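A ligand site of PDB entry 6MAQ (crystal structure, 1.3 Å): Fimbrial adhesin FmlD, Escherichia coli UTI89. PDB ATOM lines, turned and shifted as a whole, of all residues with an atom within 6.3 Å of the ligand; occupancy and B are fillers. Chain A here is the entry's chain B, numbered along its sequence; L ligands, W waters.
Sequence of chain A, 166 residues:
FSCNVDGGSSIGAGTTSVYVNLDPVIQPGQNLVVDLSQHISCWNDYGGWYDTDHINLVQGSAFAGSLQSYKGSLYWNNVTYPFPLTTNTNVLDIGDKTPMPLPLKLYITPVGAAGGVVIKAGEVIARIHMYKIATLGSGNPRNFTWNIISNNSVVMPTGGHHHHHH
O5 of the ligand sits at hydrogen-bond distance from OG of Ser 2 (2.8 Å).
The backbone NH (N) of Gly 12 lies within hydrogen-bond range of an oxygen (O4) of the ligand, 3.0 Å away.
NE of Arg 142 sits at hydrogen-bond distance from O7 of the ligand (2.8 Å).
An oxygen (O9) of the ligand is in hydrogen-bond range of the side-chain amide oxygen (OD1) of Asn 140 (3.2 Å).
An oxygen (O1) of the ligand is in hydrogen-bond range of the backbone NH (N) of Phe 1 (2.9 Å).
An oxygen (O10) of the ligand is in hydrogen-bond range of the side-chain carboxylate (OD1) of Asp 53, at 2.6 Å.
O9 of the ligand sits at hydrogen-bond distance from NZ of Lys 132 (2.9 Å).
The backbone NH (N) of Asp 45 sits at hydrogen-bond distance from an oxygen (O1) of the ligand (3.0 Å).
The backbone carbonyl oxygen (O) of Asp 53 is in hydrogen-bond range of the backbone NH (N) of Ile 94 (2.8 Å).
OD1 of Asn 44 lies within hydrogen-bond range of N of Gly 47 (2.8 Å).
The backbone carbonyl oxygen (O) of Asp 51 sits at hydrogen-bond distance from the side-chain amide nitrogen (ND2) of Asn 44.
OD2 of Asp 45 is in hydrogen-bond range of OG of Ser 2 (2.7 Å).
N of Arg 142 sits at hydrogen-bond distance from O of Lys 132.
The side-chain amide nitrogen (ND2) of Asn 44 is in hydrogen-bond range of the backbone carbonyl oxygen (O) of Tyr 50, 3.1 Å away.
N of Phe 1 sits at hydrogen-bond distance from OD2 of Asp 45 (2.8 Å).
The side-chain amide oxygen (OD1) of Asn 44 is in hydrogen-bond range of the backbone NH (N) of Tyr 46 (2.8 Å).
Water W2 lies within hydrogen-bond range of an oxygen (O8) of the ligand (2.8 Å), the side-chain amino group of Lys 132 (2.9 Å) and the backbone NH of Phe 1 (3.0 Å).
Water W4 lies within hydrogen-bond range of N2 of the ligand and OH of Tyr 46.
Merely in contact with the ligand: Ser 10 (3.9 Å), Ile 11 (3.5 Å), Asn 44 (3.3 Å), Tyr 46 (3.6 Å), Asp 51 (3.5 Å), Ala 134 (3.6 Å) and Gly 139 (3.6 Å).
Hydrophobic or aromatic side chains within 4 Å of the ligand: Phe 1, Tyr 46 and Ala 134.
Of the 26 residues printed, 15 come within 4 Å of the ligand.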
ATOM      1  N   PHE A   1      12.927 -24.040  -0.208  1.00  0.00           N
ATOM      2  CA  PHE A   1      13.645 -22.808  -0.632  1.00  0.00           C
ATOM      3  C   PHE A   1      14.650 -23.156  -1.724  1.00  0.00           C
ATOM      4  O   PHE A   1      15.309 -24.192  -1.623  1.00  0.00           O
ATOM      5  CB  PHE A   1      14.365 -22.201   0.562  1.00  0.00           C
ATOM      6  CG  PHE A   1      15.167 -20.990   0.225  1.00  0.00           C
ATOM      7  CD1 PHE A   1      16.543 -21.074   0.103  1.00  0.00           C
ATOM      8  CD2 PHE A   1      14.553 -19.760   0.001  1.00  0.00           C
ATOM      9  CE1 PHE A   1      17.305 -19.970  -0.224  1.00  0.00           C
ATOM     10  CE2 PHE A   1      15.312 -18.653  -0.312  1.00  0.00           C
ATOM     11  CZ  PHE A   1      16.693 -18.767  -0.430  1.00  0.00           C
ATOM     12  N   SER A   2      14.725 -22.331  -2.754  1.00  0.00           N
ATOM     13  CA  SER A   2      15.655 -22.577  -3.844  1.00  0.00           C
ATOM     14  C   SER A   2      16.127 -21.283  -4.451  1.00  0.00           C
ATOM     15  O   SER A   2      15.463 -20.259  -4.356  1.00  0.00           O
ATOM     16  CB  SER A   2      14.975 -23.323  -4.990  1.00  0.00           C
ATOM     17  OG  SER A   2      14.241 -24.432  -4.593  1.00  0.00           O
ATOM     18  N   CYS A   3      17.265 -21.338  -5.127  1.00  0.00           N
ATOM     19  CA  CYS A   3      17.824 -20.241  -5.894  1.00  0.00           C
ATOM     20  C   CYS A   3      18.292 -20.715  -7.272  1.00  0.00           C
ATOM     21  O   CYS A   3      18.442 -21.932  -7.501  1.00  0.00           O
ATOM     22  CB  CYS A   3      19.042 -19.662  -5.164  1.00  0.00           C
ATOM     23  SG  CYS A   3      18.765 -19.177  -3.450  1.00  0.00           S
ATOM     24  N   SER A  10      18.012 -25.208 -10.392  1.00  0.00           N
ATOM     25  CA  SER A  10      17.685 -24.828  -9.030  1.00  0.00           C
ATOM     26  C   SER A  10      18.698 -25.353  -8.035  1.00  0.00           C
ATOM     27  O   SER A  10      19.282 -26.435  -8.198  1.00  0.00           O
ATOM     28  CB  SER A  10      16.283 -25.336  -8.693  1.00  0.00           C
ATOM     29  OG  SER A  10      15.361 -24.707  -9.517  1.00  0.00           O
ATOM     30  N   ILE A  11      18.928 -24.567  -6.984  1.00  0.00           N
ATOM     31  CA  ILE A  11      19.970 -24.816  -6.004  1.00  0.00           C
ATOM     32  C   ILE A  11      19.349 -24.754  -4.624  1.00  0.00           C
ATOM     33  O   ILE A  11      18.775 -23.707  -4.252  1.00  0.00           O
ATOM     34  CB  ILE A  11      21.068 -23.725  -6.084  1.00  0.00           C
ATOM     35  CG1 ILE A  11      21.645 -23.602  -7.505  1.00  0.00           C
ATOM     36  CG2 ILE A  11      22.183 -24.000  -5.075  1.00  0.00           C
ATOM     37  CD1 ILE A  11      22.303 -22.235  -7.742  1.00  0.00           C
ATOM     38  N   GLY A  12      19.451 -25.825  -3.842  1.00  0.00           N
ATOM     39  CA  GLY A  12      18.880 -25.880  -2.509  1.00  0.00           C
ATOM     40  C   GLY A  12      19.900 -25.819  -1.391  1.00  0.00           C
ATOM     41  O   GLY A  12      19.543 -25.638  -0.228  1.00  0.00           O
ATOM     42  N   ALA A  13      21.175 -25.940  -1.740  1.00  0.00           N
ATOM     43  CA  ALA A  13      22.279 -25.865  -0.792  1.00  0.00           C
ATOM     44  C   ALA A  13      23.566 -25.989  -1.565  1.00  0.00           C
ATOM     45  O   ALA A  13      23.531 -26.322  -2.757  1.00  0.00           O
ATOM     46  CB  ALA A  13      22.201 -27.016   0.235  1.00  0.00           C
ATOM     47  N   TRP A  43      13.640 -18.068  -4.196  1.00  0.00           N
ATOM     48  CA  TRP A  43      12.188 -18.112  -4.001  1.00  0.00           C
ATOM     49  C   TRP A  43      11.828 -19.149  -2.960  1.00  0.00           C
ATOM     50  O   TRP A  43      12.590 -20.044  -2.604  1.00  0.00           O
ATOM     51  CB  TRP A  43      11.476 -18.389  -5.330  1.00  0.00           C
ATOM     52  CG  TRP A  43      11.882 -19.685  -5.928  1.00  0.00           C
ATOM     53  CD1 TRP A  43      11.281 -20.887  -5.730  1.00  0.00           C
ATOM     54  CD2 TRP A  43      12.992 -19.926  -6.804  1.00  0.00           C
ATOM     55  NE1 TRP A  43      11.960 -21.885  -6.419  1.00  0.00           N
ATOM     56  CE2 TRP A  43      13.011 -21.306  -7.094  1.00  0.00           C
ATOM     57  CE3 TRP A  43      13.983 -19.104  -7.365  1.00  0.00           C
ATOM     58  CZ2 TRP A  43      13.983 -21.875  -7.912  1.00  0.00           C
ATOM     59  CZ3 TRP A  43      14.942 -19.678  -8.177  1.00  0.00           C
ATOM     60  CH2 TRP A  43      14.928 -21.049  -8.444  1.00  0.00           C
ATOM     61  N   ASN A  44      10.589 -19.008  -2.507  1.00  0.00           N
ATOM     62  CA  ASN A  44       9.961 -19.953  -1.607  1.00  0.00           C
ATOM     63  C   ASN A  44       9.247 -21.013  -2.458  1.00  0.00           C
ATOM     64  O   ASN A  44       8.602 -20.682  -3.449  1.00  0.00           O
ATOM     65  CB  ASN A  44       8.994 -19.182  -0.673  1.00  0.00           C
ATOM     66  CG  ASN A  44       8.150 -20.080   0.210  1.00  0.00           C
ATOM     67  OD1 ASN A  44       7.313 -20.841  -0.285  1.00  0.00           O
ATOM     68  ND2 ASN A  44       8.315 -19.946   1.522  1.00  0.00           N
ATOM     69  N   ASP A  45       9.442 -22.277  -2.102  1.00  0.00           N
ATOM     70  CA  ASP A  45       8.982 -23.373  -2.968  1.00  0.00           C
ATOM     71  C   ASP A  45       7.501 -23.701  -2.828  1.00  0.00           C
ATOM     72  O   ASP A  45       6.984 -24.475  -3.635  1.00  0.00           O
ATOM     73  CB  ASP A  45       9.855 -24.620  -2.767  1.00  0.00           C
ATOM     74  CG  ASP A  45      11.177 -24.507  -3.505  1.00  0.00           C
ATOM     75  OD1 ASP A  45      11.152 -24.273  -4.729  1.00  0.00           O
ATOM     76  OD2 ASP A  45      12.222 -24.619  -2.820  1.00  0.00           O
ATOM     77  N   TYR A  46       6.827 -23.106  -1.861  1.00  0.00           N
ATOM     78  CA  TYR A  46       5.372 -23.238  -1.732  1.00  0.00           C
ATOM     79  C   TYR A  46       4.639 -22.051  -2.322  1.00  0.00           C
ATOM     80  O   TYR A  46       3.539 -22.188  -2.877  1.00  0.00           O
ATOM     81  CB  TYR A  46       4.994 -23.358  -0.275  1.00  0.00           C
ATOM     82  CG  TYR A  46       5.481 -24.600   0.431  1.00  0.00           C
ATOM     83  CD1 TYR A  46       5.365 -25.858  -0.142  1.00  0.00           C
ATOM     84  CD2 TYR A  46       6.064 -24.504   1.674  1.00  0.00           C
ATOM     85  CE1 TYR A  46       5.795 -26.984   0.531  1.00  0.00           C
ATOM     86  CE2 TYR A  46       6.487 -25.606   2.350  1.00  0.00           C
ATOM     87  CZ  TYR A  46       6.362 -26.847   1.787  1.00  0.00           C
ATOM     88  OH  TYR A  46       6.813 -27.936   2.494  1.00  0.00           O
ATOM     89  N   GLY A  47       5.222 -20.863  -2.189  1.00  0.00           N
ATOM     90  CA  GLY A  47       4.520 -19.635  -2.506  1.00  0.00           C
ATOM     91  C   GLY A  47       3.588 -19.189  -1.382  1.00  0.00           C
ATOM     92  O   GLY A  47       3.395 -19.902  -0.393  1.00  0.00           O
ATOM     93  N   TYR A  50       3.919 -19.206   2.666  1.00  0.00           N
ATOM     94  CA  TYR A  50       3.730 -20.392   3.466  1.00  0.00           C
ATOM     95  C   TYR A  50       5.100 -20.975   3.829  1.00  0.00           C
ATOM     96  O   TYR A  50       5.919 -21.240   2.950  1.00  0.00           O
ATOM     97  CB  TYR A  50       2.905 -21.421   2.695  1.00  0.00           C
ATOM     98  CG  TYR A  50       2.416 -22.525   3.582  1.00  0.00           C
ATOM     99  CD1 TYR A  50       1.228 -22.377   4.287  1.00  0.00           C
ATOM    100  CD2 TYR A  50       3.143 -23.680   3.769  1.00  0.00           C
ATOM    101  CE1 TYR A  50       0.770 -23.347   5.130  1.00  0.00           C
ATOM    102  CE2 TYR A  50       2.685 -24.675   4.645  1.00  0.00           C
ATOM    103  CZ  TYR A  50       1.499 -24.480   5.321  1.00  0.00           C
ATOM    104  OH  TYR A  50       1.008 -25.449   6.181  1.00  0.00           O
ATOM    105  N   ASP A  51       5.358 -21.167   5.117  1.00  0.00           N
ATOM    106  CA  ASP A  51       6.675 -21.589   5.586  1.00  0.00           C
ATOM    107  C   ASP A  51       7.750 -20.639   5.083  1.00  0.00           C
ATOM    108  O   ASP A  51       8.664 -21.026   4.359  1.00  0.00           O
ATOM    109  CB  ASP A  51       6.965 -23.022   5.171  1.00  0.00           C
ATOM    110  CG  ASP A  51       8.030 -23.675   6.034  1.00  0.00           C
ATOM    111  OD1 ASP A  51       8.481 -23.056   7.013  1.00  0.00           O
ATOM    112  OD2 ASP A  51       8.402 -24.830   5.713  1.00  0.00           O
ATOM    113  N   THR A  52       7.639 -19.380   5.485  1.00  0.00           N
ATOM    114  CA  THR A  52       8.510 -18.321   5.016  1.00  0.00           C
ATOM    115  C   THR A  52       9.960 -18.622   5.319  1.00  0.00           C
ATOM    116  O   THR A  52      10.318 -19.113   6.386  1.00  0.00           O
ATOM    117  CB  THR A  52       8.066 -16.969   5.593  1.00  0.00           C
ATOM    118  OG1 THR A  52       6.805 -16.597   5.039  1.00  0.00           O
ATOM    119  CG2 THR A  52       9.028 -15.855   5.244  1.00  0.00           C
ATOM    120  N   ASP A  53      10.799 -18.338   4.332  1.00  0.00           N
ATOM    121  CA  ASP A  53      12.252 -18.551   4.407  1.00  0.00           C
ATOM    122  C   ASP A  53      12.957 -17.324   4.942  1.00  0.00           C
ATOM    123  O   ASP A  53      12.612 -16.204   4.600  1.00  0.00           O
ATOM    124  CB  ASP A  53      12.761 -18.918   3.019  1.00  0.00           C
ATOM    125  CG  ASP A  53      12.157 -20.232   2.526  1.00  0.00           C
ATOM    126  OD1 ASP A  53      12.419 -21.235   3.228  1.00  0.00           O
ATOM    127  OD2 ASP A  53      11.454 -20.221   1.495  1.00  0.00           O
ATOM    128  N   ILE A  94      11.759 -14.445   2.548  1.00  0.00           N
ATOM    129  CA  ILE A  94      11.362 -14.830   1.196  1.00  0.00           C
ATOM    130  C   ILE A  94      10.151 -15.763   1.256  1.00  0.00           C
ATOM    131  O   ILE A  94      10.196 -16.784   1.943  1.00  0.00           O
ATOM    132  CB  ILE A  94      12.547 -15.469   0.441  1.00  0.00           C
ATOM    133  CG1 ILE A  94      13.579 -14.360   0.161  1.00  0.00           C
ATOM    134  CG2 ILE A  94      12.093 -16.125  -0.851  1.00  0.00           C
ATOM    135  CD1 ILE A  94      14.809 -14.747  -0.660  1.00  0.00           C
ATOM    136  N   LYS A 132      20.050 -20.284   5.275  1.00  0.00           N
ATOM    137  CA  LYS A 132      18.593 -20.315   5.157  1.00  0.00           C
ATOM    138  C   LYS A 132      18.016 -21.148   6.287  1.00  0.00           C
ATOM    139  O   LYS A 132      18.489 -22.241   6.572  1.00  0.00           O
ATOM    140  CB  LYS A 132      18.185 -20.927   3.822  1.00  0.00           C
ATOM    141  CG  LYS A 132      16.692 -21.317   3.731  1.00  0.00           C
ATOM    142  CD  LYS A 132      16.444 -22.813   3.918  1.00  0.00           C
ATOM    143  CE  LYS A 132      14.966 -23.120   4.178  1.00  0.00           C
ATOM    144  NZ  LYS A 132      14.682 -24.604   4.170  1.00  0.00           N
ATOM    145  N   ILE A 133      16.964 -20.628   6.928  1.00  0.00           N
ATOM    146  CA  ILE A 133      16.127 -21.441   7.799  1.00  0.00           C
ATOM    147  C   ILE A 133      14.694 -20.952   7.578  1.00  0.00           C
ATOM    148  O   ILE A 133      14.467 -19.746   7.415  1.00  0.00           O
ATOM    149  CB  ILE A 133      16.571 -21.362   9.284  1.00  0.00           C
ATOM    150  CG1 ILE A 133      15.806 -22.390  10.119  1.00  0.00           C
ATOM    151  CG2 ILE A 133      16.430 -19.957   9.826  1.00  0.00           C
ATOM    152  CD1 ILE A 133      16.373 -22.567  11.538  1.00  0.00           C
ATOM    153  N   ALA A 134      13.739 -21.874   7.545  1.00  0.00           N
ATOM    154  CA  ALA A 134      12.353 -21.490   7.311  1.00  0.00           C
ATOM    155  C   ALA A 134      11.628 -21.355   8.650  1.00  0.00           C
ATOM    156  O   ALA A 134      12.246 -21.031   9.676  1.00  0.00           O
ATOM    157  CB  ALA A 134      11.670 -22.482   6.353  1.00  0.00           C
ATOM    158  N   THR A 135      10.318 -21.602   8.658  1.00  0.00           N
ATOM    159  CA  THR A 135       9.449 -21.212   9.772  1.00  0.00           C
ATOM    160  C   THR A 135       8.841 -22.400  10.495  1.00  0.00           C
ATOM    161  O   THR A 135       8.752 -22.386  11.730  1.00  0.00           O
ATOM    162  CB  THR A 135       8.339 -20.292   9.252  1.00  0.00           C
ATOM    163  OG1 THR A 135       8.921 -19.087   8.754  1.00  0.00           O
ATOM    164  CG2 THR A 135       7.344 -19.922  10.364  1.00  0.00           C
ATOM    165  N   LEU A 136       8.437 -23.413   9.748  1.00  0.00           N
ATOM    166  CA  LEU A 136       7.711 -24.555  10.302  1.00  0.00           C
ATOM    167  C   LEU A 136       8.652 -25.714  10.616  1.00  0.00           C
ATOM    168  O   LEU A 136       9.660 -25.941   9.925  1.00  0.00           O
ATOM    169  CB  LEU A 136       6.609 -25.004   9.331  1.00  0.00           C
ATOM    170  CG  LEU A 136       5.585 -23.940   8.933  1.00  0.00           C
ATOM    171  CD1 LEU A 136       4.600 -24.525   7.921  1.00  0.00           C
ATOM    172  CD2 LEU A 136       4.843 -23.376  10.141  1.00  0.00           C
ATOM    173  N   GLY A 139      12.586 -25.926  10.401  1.00  0.00           N
ATOM    174  CA  GLY A 139      12.979 -24.906   9.447  1.00  0.00           C
ATOM    175  C   GLY A 139      13.909 -25.399   8.351  1.00  0.00           C
ATOM    176  O   GLY A 139      14.239 -24.638   7.440  1.00  0.00           O
ATOM    177  N   ASN A 140      14.337 -26.662   8.430  1.00  0.00           N
ATOM    178  CA  ASN A 140      15.208 -27.285   7.424  1.00  0.00           C
ATOM    179  C   ASN A 140      16.371 -26.384   7.014  1.00  0.00           C
ATOM    180  O   ASN A 140      16.461 -25.954   5.857  1.00  0.00           O
ATOM    181  CB  ASN A 140      14.387 -27.715   6.217  1.00  0.00           C
ATOM    182  CG  ASN A 140      13.327 -28.721   6.579  1.00  0.00           C
ATOM    183  OD1 ASN A 140      12.132 -28.442   6.504  1.00  0.00           O
ATOM    184  ND2 ASN A 140      13.751 -29.897   7.005  1.00  0.00           N
ATOM    185  N   PRO A 141      17.261 -26.107   7.972  1.00  0.00           N
ATOM    186  CA  PRO A 141      18.349 -25.187   7.656  1.00  0.00           C
ATOM    187  C   PRO A 141      19.229 -25.663   6.507  1.00  0.00           C
ATOM    188  O   PRO A 141      19.493 -26.864   6.350  1.00  0.00           O
ATOM    189  CB  PRO A 141      19.130 -25.055   8.974  1.00  0.00           C
ATOM    190  CG  PRO A 141      18.644 -26.161   9.848  1.00  0.00           C
ATOM    191  CD  PRO A 141      17.294 -26.581   9.378  1.00  0.00           C
ATOM    192  N   ARG A 142      19.710 -24.708   5.698  1.00  0.00           N
ATOM    193  CA  ARG A 142      20.570 -24.997   4.554  1.00  0.00           C
ATOM    194  C   ARG A 142      21.675 -23.972   4.479  1.00  0.00           C
ATOM    195  O   ARG A 142      21.481 -22.793   4.808  1.00  0.00           O
ATOM    196  CB  ARG A 142      19.776 -24.943   3.258  1.00  0.00           C
ATOM    197  CG  ARG A 142      18.637 -25.959   3.175  1.00  0.00           C
ATOM    198  CD  ARG A 142      19.122 -27.377   3.011  1.00  0.00           C
ATOM    199  NE  ARG A 142      18.029 -28.340   2.841  1.00  0.00           N
ATOM    200  CZ  ARG A 142      17.524 -29.106   3.799  1.00  0.00           C
ATOM    201  NH1 ARG A 142      17.965 -29.047   5.048  1.00  0.00           N
ATOM    202  NH2 ARG A 142      16.544 -29.953   3.505  1.00  0.00           N
HETATM  203  N1  LIG L   1      15.791 -29.350   0.094  1.00  0.00           N
HETATM  204  C1  LIG L   1       9.508 -23.045   1.426  1.00  0.00           C
HETATM  205  O1  LIG L   1      10.581 -22.538   0.614  1.00  0.00           O
HETATM  206  C2  LIG L   1       9.862 -24.382   2.033  1.00  0.00           C
HETATM  207  C3  LIG L   1      13.492 -27.655  -3.117  1.00  0.00           C
HETATM  208  C4  LIG L   1      14.826 -27.730  -3.168  1.00  0.00           C
HETATM  209  C5  LIG L   1      15.515 -27.243  -4.395  1.00  0.00           C
HETATM  210  C6  LIG L   1      15.622 -28.323  -2.057  1.00  0.00           C
HETATM  211  C7  LIG L   1      15.010 -28.790  -0.958  1.00  0.00           C
HETATM  212  C8  LIG L   1      13.489 -28.714  -0.899  1.00  0.00           C
HETATM  213  C9  LIG L   1      11.595 -26.581   2.561  1.00  0.00           C
HETATM  214  C10 LIG L   1      12.972 -28.640   2.908  1.00  0.00           C
HETATM  215  C11 LIG L   1      12.954 -30.091   3.353  1.00  0.00           C
HETATM  216  C12 LIG L   1      11.093 -25.716   3.694  1.00  0.00           C
HETATM  217  C13 LIG L   1      10.622 -26.526   1.404  1.00  0.00           C
HETATM  218  C14 LIG L   1      10.871 -24.308   3.169  1.00  0.00           C
HETATM  219  C15 LIG L   1      10.504 -27.572  -0.777  1.00  0.00           C
HETATM  220  C16 LIG L   1       9.113 -27.472  -0.789  1.00  0.00           C
HETATM  221  C17 LIG L   1       8.461 -27.868  -1.932  1.00  0.00           C
HETATM  222  C18 LIG L   1       9.127 -28.340  -3.027  1.00  0.00           C
HETATM  223  C19 LIG L   1      10.499 -28.436  -3.019  1.00  0.00           C
HETATM  224  C20 LIG L   1      11.232 -28.065  -1.896  1.00  0.00           C
HETATM  225  C21 LIG L   1      12.760 -28.173  -1.912  1.00  0.00           C
HETATM  226  N2  LIG L   1      11.752 -27.947   2.970  1.00  0.00           N
HETATM  227  O2  LIG L   1      10.345 -25.203   0.992  1.00  0.00           O
HETATM  228  O3  LIG L   1      11.256 -27.204   0.349  1.00  0.00           O
HETATM  229  O4  LIG L   1      16.768 -27.078  -4.393  1.00  0.00           O
HETATM  230  O5  LIG L   1      14.847 -27.029  -5.430  1.00  0.00           O
HETATM  231  O6  LIG L   1      15.374 -30.312   0.711  1.00  0.00           O
HETATM  232  O7  LIG L   1      16.908 -28.890   0.343  1.00  0.00           O
HETATM  233  O8  LIG L   1      14.012 -28.117   2.536  1.00  0.00           O
HETATM  234  O9  LIG L   1      12.038 -25.734   4.755  1.00  0.00           O
HETATM  235  O10 LIG L   1      12.127 -23.766   2.761  1.00  0.00           O
HETATM  236  O   HOH W   1      13.249 -31.664  -0.068  1.00  0.00           O
HETATM  237  O   HOH W   2      14.809 -25.652   1.520  1.00  0.00           O
HETATM  238  O   HOH W   3      10.510 -25.780   7.093  1.00  0.00           O
HETATM  239  O   HOH W   4       9.350 -29.103   4.151  1.00  0.00           O
